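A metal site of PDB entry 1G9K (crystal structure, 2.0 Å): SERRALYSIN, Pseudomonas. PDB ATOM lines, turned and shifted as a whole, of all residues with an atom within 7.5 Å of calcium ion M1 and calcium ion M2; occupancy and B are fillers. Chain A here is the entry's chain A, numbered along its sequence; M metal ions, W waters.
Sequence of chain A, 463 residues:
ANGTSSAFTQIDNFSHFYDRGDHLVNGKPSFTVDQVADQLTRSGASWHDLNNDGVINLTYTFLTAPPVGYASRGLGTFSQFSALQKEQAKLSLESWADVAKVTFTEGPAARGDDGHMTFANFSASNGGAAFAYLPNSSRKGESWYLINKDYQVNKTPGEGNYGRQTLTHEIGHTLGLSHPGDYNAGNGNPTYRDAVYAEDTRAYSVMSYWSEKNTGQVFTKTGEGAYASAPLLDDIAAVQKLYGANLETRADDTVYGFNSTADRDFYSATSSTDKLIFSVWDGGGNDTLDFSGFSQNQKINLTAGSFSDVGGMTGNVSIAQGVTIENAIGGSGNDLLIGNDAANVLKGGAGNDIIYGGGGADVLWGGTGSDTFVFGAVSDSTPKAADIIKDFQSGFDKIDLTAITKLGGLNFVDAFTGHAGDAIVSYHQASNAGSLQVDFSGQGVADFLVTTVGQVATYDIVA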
ATOM      1  N   LEU A 302      10.340  10.648   4.827  1.00  0.00           N
ATOM      2  CA  LEU A 302      11.619  11.240   5.201  1.00  0.00           C
ATOM      3  C   LEU A 302      11.466  12.422   6.160  1.00  0.00           C
ATOM      4  O   LEU A 302      12.436  13.123   6.431  1.00  0.00           O
ATOM      5  CB  LEU A 302      12.393  11.681   3.942  1.00  0.00           C
ATOM      6  CG  LEU A 302      12.825  10.560   2.986  1.00  0.00           C
ATOM      7  CD1 LEU A 302      13.637  11.142   1.824  1.00  0.00           C
ATOM      8  CD2 LEU A 302      13.657   9.541   3.747  1.00  0.00           C
ATOM      9  N   GLU A 326      18.183  12.742   3.401  1.00  0.00           N
ATOM     10  CA  GLU A 326      17.959  13.214   2.037  1.00  0.00           C
ATOM     11  C   GLU A 326      17.346  12.281   0.999  1.00  0.00           C
ATOM     12  O   GLU A 326      16.493  12.698   0.205  1.00  0.00           O
ATOM     13  CB  GLU A 326      19.284  13.746   1.459  1.00  0.00           C
ATOM     14  CG  GLU A 326      19.858  14.979   2.150  1.00  0.00           C
ATOM     15  CD  GLU A 326      20.322  14.731   3.571  1.00  0.00           C
ATOM     16  OE1 GLU A 326      20.725  13.598   3.908  1.00  0.00           O
ATOM     17  OE2 GLU A 326      20.288  15.690   4.371  1.00  0.00           O
ATOM     18  N   ILE A 338       7.617   9.667   0.546  1.00  0.00           N
ATOM     19  CA  ILE A 338       7.374  11.058   0.907  1.00  0.00           C
ATOM     20  C   ILE A 338       8.693  11.713   1.293  1.00  0.00           C
ATOM     21  O   ILE A 338       9.368  11.283   2.231  1.00  0.00           O
ATOM     22  CB  ILE A 338       6.412  11.156   2.096  1.00  0.00           C
ATOM     23  CG1 ILE A 338       5.110  10.422   1.758  1.00  0.00           C
ATOM     24  CG2 ILE A 338       6.123  12.617   2.422  1.00  0.00           C
ATOM     25  CD1 ILE A 338       4.103  10.401   2.880  1.00  0.00           C
ATOM     26  N   GLY A 339       9.057  12.753   0.550  1.00  0.00           N
ATOM     27  CA  GLY A 339      10.299  13.461   0.837  1.00  0.00           C
ATOM     28  C   GLY A 339      10.038  14.558   1.846  1.00  0.00           C
ATOM     29  O   GLY A 339       8.948  14.638   2.416  1.00  0.00           O
ATOM     30  N   ASN A 340      11.042  15.403   2.060  1.00  0.00           N
ATOM     31  CA  ASN A 340      10.911  16.512   2.994  1.00  0.00           C
ATOM     32  C   ASN A 340      11.252  17.833   2.292  1.00  0.00           C
ATOM     33  O   ASN A 340      11.343  17.881   1.061  1.00  0.00           O
ATOM     34  CB  ASN A 340      11.836  16.299   4.196  1.00  0.00           C
ATOM     35  CG  ASN A 340      13.229  15.857   3.802  1.00  0.00           C
ATOM     36  OD1 ASN A 340      13.824  16.389   2.862  1.00  0.00           O
ATOM     37  ND2 ASN A 340      13.765  14.872   4.526  1.00  0.00           N
ATOM     38  N   ASP A 341      11.453  18.884   3.077  1.00  0.00           N
ATOM     39  CA  ASP A 341      11.768  20.216   2.543  1.00  0.00           C
ATOM     40  C   ASP A 341      13.108  20.294   1.830  1.00  0.00           C
ATOM     41  O   ASP A 341      13.362  21.252   1.086  1.00  0.00           O
ATOM     42  CB  ASP A 341      11.753  21.246   3.678  1.00  0.00           C
ATOM     43  CG  ASP A 341      10.365  21.513   4.207  1.00  0.00           C
ATOM     44  OD1 ASP A 341      10.243  22.200   5.249  1.00  0.00           O
ATOM     45  OD2 ASP A 341       9.396  21.032   3.576  1.00  0.00           O
ATOM     46  N   ALA A 342      13.967  19.312   2.045  1.00  0.00           N
ATOM     47  CA  ALA A 342      15.267  19.322   1.401  1.00  0.00           C
ATOM     48  C   ALA A 342      15.195  18.700   0.015  1.00  0.00           C
ATOM     49  O   ALA A 342      14.183  18.093  -0.351  1.00  0.00           O
ATOM     50  CB  ALA A 342      16.275  18.583   2.270  1.00  0.00           C
ATOM     51  N   ALA A 343      16.264  18.878  -0.752  1.00  0.00           N
ATOM     52  CA  ALA A 343      16.343  18.307  -2.089  1.00  0.00           C
ATOM     53  C   ALA A 343      16.575  16.813  -1.895  1.00  0.00           C
ATOM     54  O   ALA A 343      17.613  16.410  -1.370  1.00  0.00           O
ATOM     55  CB  ALA A 343      17.507  18.926  -2.856  1.00  0.00           C
ATOM     56  N   ASN A 344      15.608  16.013  -2.318  1.00  0.00           N
ATOM     57  CA  ASN A 344      15.686  14.563  -2.142  1.00  0.00           C
ATOM     58  C   ASN A 344      15.847  13.800  -3.448  1.00  0.00           C
ATOM     59  O   ASN A 344      15.446  14.264  -4.510  1.00  0.00           O
ATOM     60  CB  ASN A 344      14.415  14.030  -1.477  1.00  0.00           C
ATOM     61  CG  ASN A 344      13.961  14.860  -0.295  1.00  0.00           C
ATOM     62  OD1 ASN A 344      12.826  15.356  -0.280  1.00  0.00           O
ATOM     63  ND2 ASN A 344      14.821  15.012   0.708  1.00  0.00           N
ATOM     64  N   VAL A 345      16.440  12.613  -3.351  1.00  0.00           N
ATOM     65  CA  VAL A 345      16.567  11.733  -4.508  1.00  0.00           C
ATOM     66  C   VAL A 345      15.659  10.578  -4.089  1.00  0.00           C
ATOM     67  O   VAL A 345      15.940   9.891  -3.111  1.00  0.00           O
ATOM     68  CB  VAL A 345      18.002  11.215  -4.689  1.00  0.00           C
ATOM     69  CG1 VAL A 345      18.028  10.174  -5.806  1.00  0.00           C
ATOM     70  CG2 VAL A 345      18.944  12.366  -5.044  1.00  0.00           C
ATOM     71  N   LEU A 346      14.553  10.386  -4.807  1.00  0.00           N
ATOM     72  CA  LEU A 346      13.607   9.316  -4.486  1.00  0.00           C
ATOM     73  C   LEU A 346      13.452   8.332  -5.638  1.00  0.00           C
ATOM     74  O   LEU A 346      13.100   8.712  -6.759  1.00  0.00           O
ATOM     75  CB  LEU A 346      12.244   9.924  -4.151  1.00  0.00           C
ATOM     76  CG  LEU A 346      12.223  11.033  -3.086  1.00  0.00           C
ATOM     77  CD1 LEU A 346      10.838  11.669  -3.001  1.00  0.00           C
ATOM     78  CD2 LEU A 346      12.615  10.429  -1.734  1.00  0.00           C
ATOM     79  N   TYR A 356       6.284  11.640  -3.698  1.00  0.00           N
ATOM     80  CA  TYR A 356       6.000  13.012  -3.312  1.00  0.00           C
ATOM     81  C   TYR A 356       7.308  13.666  -2.904  1.00  0.00           C
ATOM     82  O   TYR A 356       7.844  13.376  -1.833  1.00  0.00           O
ATOM     83  CB  TYR A 356       5.053  13.008  -2.112  1.00  0.00           C
ATOM     84  CG  TYR A 356       4.405  14.338  -1.817  1.00  0.00           C
ATOM     85  CD1 TYR A 356       3.220  14.713  -2.451  1.00  0.00           C
ATOM     86  CD2 TYR A 356       4.962  15.218  -0.885  1.00  0.00           C
ATOM     87  CE1 TYR A 356       2.601  15.920  -2.167  1.00  0.00           C
ATOM     88  CE2 TYR A 356       4.345  16.435  -0.591  1.00  0.00           C
ATOM     89  CZ  TYR A 356       3.165  16.770  -1.237  1.00  0.00           C
ATOM     90  OH  TYR A 356       2.534  17.962  -0.929  1.00  0.00           O
ATOM     91  N   GLY A 357       7.835  14.546  -3.757  1.00  0.00           N
ATOM     92  CA  GLY A 357       9.083  15.205  -3.456  1.00  0.00           C
ATOM     93  C   GLY A 357       9.011  16.286  -2.384  1.00  0.00           C
ATOM     94  O   GLY A 357       9.969  16.482  -1.630  1.00  0.00           O
ATOM     95  N   GLY A 358       7.885  16.973  -2.292  1.00  0.00           N
ATOM     96  CA  GLY A 358       7.757  18.032  -1.314  1.00  0.00           C
ATOM     97  C   GLY A 358       8.576  19.253  -1.716  1.00  0.00           C
ATOM     98  O   GLY A 358       8.893  19.425  -2.891  1.00  0.00           O
ATOM     99  N   GLY A 359       8.920  20.089  -0.738  1.00  0.00           N
ATOM    100  CA  GLY A 359       9.703  21.273  -1.024  1.00  0.00           C
ATOM    101  C   GLY A 359      11.078  20.977  -1.592  1.00  0.00           C
ATOM    102  O   GLY A 359      11.561  19.840  -1.498  1.00  0.00           O
ATOM    103  N   GLY A 360      11.714  21.989  -2.183  1.00  0.00           N
ATOM    104  CA  GLY A 360      13.031  21.816  -2.753  1.00  0.00           C
ATOM    105  C   GLY A 360      13.039  21.173  -4.126  1.00  0.00           C
ATOM    106  O   GLY A 360      12.018  20.636  -4.573  1.00  0.00           O
ATOM    107  N   ALA A 361      14.186  21.230  -4.802  1.00  0.00           N
ATOM    108  CA  ALA A 361      14.334  20.645  -6.131  1.00  0.00           C
ATOM    109  C   ALA A 361      14.719  19.185  -5.968  1.00  0.00           C
ATOM    110  O   ALA A 361      15.859  18.870  -5.648  1.00  0.00           O
ATOM    111  CB  ALA A 361      15.404  21.396  -6.911  1.00  0.00           C
ATOM    112  N   ASP A 362      13.755  18.300  -6.211  1.00  0.00           N
ATOM    113  CA  ASP A 362      13.981  16.873  -6.046  1.00  0.00           C
ATOM    114  C   ASP A 362      14.292  16.142  -7.354  1.00  0.00           C
ATOM    115  O   ASP A 362      13.885  16.560  -8.432  1.00  0.00           O
ATOM    116  CB  ASP A 362      12.760  16.233  -5.373  1.00  0.00           C
ATOM    117  CG  ASP A 362      12.409  16.914  -4.051  1.00  0.00           C
ATOM    118  OD1 ASP A 362      13.240  16.901  -3.123  1.00  0.00           O
ATOM    119  OD2 ASP A 362      11.289  17.471  -3.949  1.00  0.00           O
ATOM    120  N   VAL A 363      15.040  15.038  -7.228  1.00  0.00           N
ATOM    121  CA  VAL A 363      15.396  14.201  -8.364  1.00  0.00           C
ATOM    122  C   VAL A 363      14.580  12.944  -8.161  1.00  0.00           C
ATOM    123  O   VAL A 363      14.788  12.202  -7.205  1.00  0.00           O
ATOM    124  CB  VAL A 363      16.892  13.854  -8.365  1.00  0.00           C
ATOM    125  CG1 VAL A 363      17.233  13.041  -9.596  1.00  0.00           C
ATOM    126  CG2 VAL A 363      17.715  15.126  -8.296  1.00  0.00           C
ATOM    127  N   LEU A 364      13.629  12.708  -9.062  1.00  0.00           N
ATOM    128  CA  LEU A 364      12.734  11.567  -8.937  1.00  0.00           C
ATOM    129  C   LEU A 364      12.976  10.467  -9.969  1.00  0.00           C
ATOM    130  O   LEU A 364      13.165  10.740 -11.152  1.00  0.00           O
ATOM    131  CB  LEU A 364      11.290  12.046  -9.036  1.00  0.00           C
ATOM    132  CG  LEU A 364      10.934  13.288  -8.214  1.00  0.00           C
ATOM    133  CD1 LEU A 364       9.527  13.754  -8.557  1.00  0.00           C
ATOM    134  CD2 LEU A 364      11.042  12.964  -6.738  1.00  0.00           C
ATOM    135  N   VAL A 374       3.307  12.919  -7.413  1.00  0.00           N
ATOM    136  CA  VAL A 374       2.346  13.840  -6.825  1.00  0.00           C
ATOM    137  C   VAL A 374       2.946  15.180  -6.369  1.00  0.00           C
ATOM    138  O   VAL A 374       4.073  15.239  -5.881  1.00  0.00           O
ATOM    139  CB  VAL A 374       1.638  13.173  -5.598  1.00  0.00           C
ATOM    140  CG1 VAL A 374       0.585  14.109  -5.024  1.00  0.00           C
ATOM    141  CG2 VAL A 374       1.015  11.857  -6.023  1.00  0.00           C
ATOM    142  N   PHE A 375       2.158  16.234  -6.547  1.00  0.00           N
ATOM    143  CA  PHE A 375       2.555  17.583  -6.155  1.00  0.00           C
ATOM    144  C   PHE A 375       1.419  18.150  -5.319  1.00  0.00           C
ATOM    145  O   PHE A 375       0.270  18.170  -5.758  1.00  0.00           O
ATOM    146  CB  PHE A 375       2.802  18.440  -7.401  1.00  0.00           C
ATOM    147  CG  PHE A 375       3.996  18.003  -8.180  1.00  0.00           C
ATOM    148  CD1 PHE A 375       5.264  18.507  -7.879  1.00  0.00           C
ATOM    149  CD2 PHE A 375       3.867  17.037  -9.171  1.00  0.00           C
ATOM    150  CE1 PHE A 375       6.380  18.038  -8.548  1.00  0.00           C
ATOM    151  CE2 PHE A 375       4.994  16.565  -9.848  1.00  0.00           C
ATOM    152  CZ  PHE A 375       6.256  17.064  -9.541  1.00  0.00           C
ATOM    153  N   ALA A 377       1.683  21.317  -3.619  1.00  0.00           N
ATOM    154  CA  ALA A 377       1.746  22.772  -3.560  1.00  0.00           C
ATOM    155  C   ALA A 377       2.605  23.301  -4.704  1.00  0.00           C
ATOM    156  O   ALA A 377       3.507  22.607  -5.186  1.00  0.00           O
ATOM    157  CB  ALA A 377       2.322  23.215  -2.221  1.00  0.00           C
ATOM    158  N   SER A 379       4.789  25.549  -4.562  1.00  0.00           N
ATOM    159  CA  SER A 379       6.152  25.687  -4.049  1.00  0.00           C
ATOM    160  C   SER A 379       6.944  24.376  -4.111  1.00  0.00           C
ATOM    161  O   SER A 379       8.158  24.377  -3.906  1.00  0.00           O
ATOM    162  CB  SER A 379       6.130  26.194  -2.608  1.00  0.00           C
ATOM    163  OG  SER A 379       5.409  25.311  -1.771  1.00  0.00           O
ATOM    164  N   ASP A 380       6.273  23.267  -4.385  1.00  0.00           N
ATOM    165  CA  ASP A 380       6.955  21.978  -4.474  1.00  0.00           C
ATOM    166  C   ASP A 380       7.926  21.940  -5.652  1.00  0.00           C
ATOM    167  O   ASP A 380       8.972  21.293  -5.572  1.00  0.00           O
ATOM    168  CB  ASP A 380       5.953  20.823  -4.641  1.00  0.00           C
ATOM    169  CG  ASP A 380       5.262  20.446  -3.341  1.00  0.00           C
ATOM    170  OD1 ASP A 380       5.499  21.115  -2.318  1.00  0.00           O
ATOM    171  OD2 ASP A 380       4.470  19.489  -3.353  1.00  0.00           O
ATOM    172  N   SER A 381       7.587  22.642  -6.728  1.00  0.00           N
ATOM    173  CA  SER A 381       8.435  22.651  -7.923  1.00  0.00           C
ATOM    174  C   SER A 381       8.291  23.965  -8.693  1.00  0.00           C
ATOM    175  O   SER A 381       7.461  24.096  -9.582  1.00  0.00           O
ATOM    176  CB  SER A 381       8.057  21.473  -8.818  1.00  0.00           C
ATOM    177  OG  SER A 381       9.110  21.140  -9.700  1.00  0.00           O
ATOM    178  N   THR A 382       9.130  24.933  -8.336  1.00  0.00           N
ATOM    179  CA  THR A 382       9.122  26.251  -8.946  1.00  0.00           C
ATOM    180  C   THR A 382      10.221  26.387  -9.989  1.00  0.00           C
ATOM    181  O   THR A 382      11.162  25.591 -10.014  1.00  0.00           O
ATOM    182  CB  THR A 382       9.338  27.341  -7.873  1.00  0.00           C
ATOM    183  OG1 THR A 382      10.661  27.213  -7.335  1.00  0.00           O
ATOM    184  CG2 THR A 382       8.331  27.190  -6.749  1.00  0.00           C
ATOM    185  N   ALA A 385      13.687  26.323  -8.251  1.00  0.00           N
ATOM    186  CA  ALA A 385      14.072  24.984  -7.795  1.00  0.00           C
ATOM    187  C   ALA A 385      13.038  23.973  -8.256  1.00  0.00           C
ATOM    188  O   ALA A 385      12.155  23.575  -7.493  1.00  0.00           O
ATOM    189  CB  ALA A 385      14.179  24.976  -6.275  1.00  0.00           C
ATOM    190  N   ALA A 386      13.153  23.533  -9.506  1.00  0.00           N
ATOM    191  CA  ALA A 386      12.200  22.576 -10.071  1.00  0.00           C
ATOM    192  C   ALA A 386      12.659  21.129  -9.973  1.00  0.00           C
ATOM    193  O   ALA A 386      13.850  20.824 -10.047  1.00  0.00           O
ATOM    194  CB  ALA A 386      11.924  22.933 -11.523  1.00  0.00           C
ATOM    195  N   ASP A 387      11.688  20.240  -9.837  1.00  0.00           N
ATOM    196  CA  ASP A 387      11.926  18.814  -9.762  1.00  0.00           C
ATOM    197  C   ASP A 387      12.314  18.300 -11.136  1.00  0.00           C
ATOM    198  O   ASP A 387      12.111  18.979 -12.142  1.00  0.00           O
ATOM    199  CB  ASP A 387      10.655  18.077  -9.328  1.00  0.00           C
ATOM    200  CG  ASP A 387      10.441  18.087  -7.836  1.00  0.00           C
ATOM    201  OD1 ASP A 387      11.049  18.919  -7.129  1.00  0.00           O
ATOM    202  OD2 ASP A 387       9.656  17.249  -7.362  1.00  0.00           O
ATOM    203  N   ILE A 388      12.847  17.092 -11.171  1.00  0.00           N
ATOM    204  CA  ILE A 388      13.229  16.460 -12.418  1.00  0.00           C
ATOM    205  C   ILE A 388      12.959  14.957 -12.344  1.00  0.00           C
ATOM    206  O   ILE A 388      13.392  14.289 -11.394  1.00  0.00           O
ATOM    207  CB  ILE A 388      14.716  16.706 -12.746  1.00  0.00           C
ATOM    208  CG1 ILE A 388      15.098  15.971 -14.035  1.00  0.00           C
ATOM    209  CG2 ILE A 388      15.594  16.258 -11.582  1.00  0.00           C
ATOM    210  CD1 ILE A 388      16.514  16.248 -14.491  1.00  0.00           C
HETATM  211 CA    CA M   1      12.022  17.510  -1.169  1.00  0.00          CA
HETATM  212 CA    CA M   2      10.063  19.328  -4.929  1.00  0.00          CA
HETATM  213  O   HOH W   1       8.239  18.027  -5.413  1.00  0.00           O
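Calcium ion M2 is bound by water W1 (2.3 Å).
Calcium ion M2 is bound by O of Asp 380.
The backbone carbonyl oxygen (O) of Gly 358 binds calcium ion M2 (2.4 Å).
The backbone carbonyl oxygen (O) of Gly 360 binds calcium ion M2.
Calcium ion M2 is bound by OD2 of Asp 362.
Calcium ion M2 is bound by OD1 of Asp 387 (2.4 Å).
Six residues have an atom within 4 Å of calcium ion M2: Gly 358, Gly 359, Gly 360, Asp 362, Asp 380 and Asp 387.
Seven residues have an atom within 4 Å of calcium ion M1: Asn 340, Ala 342, Asn 344, Gly 357, Gly 358, Gly 359 and Asp 362.
The backbone carbonyl oxygen (O) of Asn 344 lies within hydrogen-bond range of the backbone NH (N) of Val 363 (2.9 Å).
ND2 of Asn 344 is in hydrogen-bond range of O of Glu 326, at 2.9 Å.
The backbone NH of Asp 387 sits at hydrogen-bond distance from the side-chain hydroxyl of Ser 381 (2.7 Å).
The side-chain amide oxygen (OD1) of Asn 340 is in hydrogen-bond range of the backbone NH (N) of Ala 342 (3.0 Å).
The backbone NH (N) of Ala 377 sits at hydrogen-bond distance from the side-chain carboxylate (OD2) of Asp 380, at 3.3 Å.
N of Ile 388 is in hydrogen-bond range of O of Asp 362 (3.0 Å).
The backbone carbonyl oxygen (O) of Leu 302 lies within hydrogen-bond range of the side-chain amide nitrogen (ND2) of Asn 340 (2.9 Å).
The side-chain hydroxyl of Tyr 356 lies within hydrogen-bond range of the side-chain carboxylate of Asp 380.
Water W1 lies within hydrogen-bond range of OD2 of Asp 387 and N of Gly 358.
Calcium ion M1 is bound by the backbone carbonyl oxygen (O) of Gly 357 (2.3 Å), the backbone carbonyl oxygen (O) of Asn 340 (2.4 Å), the side-chain carboxylate (OD1) of Asp 362 (2.4 Å), the backbone carbonyl oxygen (O) of Ala 342 (2.4 Å), the backbone carbonyl oxygen (O) of Gly 359 (2.4 Å), the side-chain amide oxygen (OD1) of Asn 344 (2.5 Å) and the side-chain carboxylate (OD2) of Asp 362 (2.9 Å).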
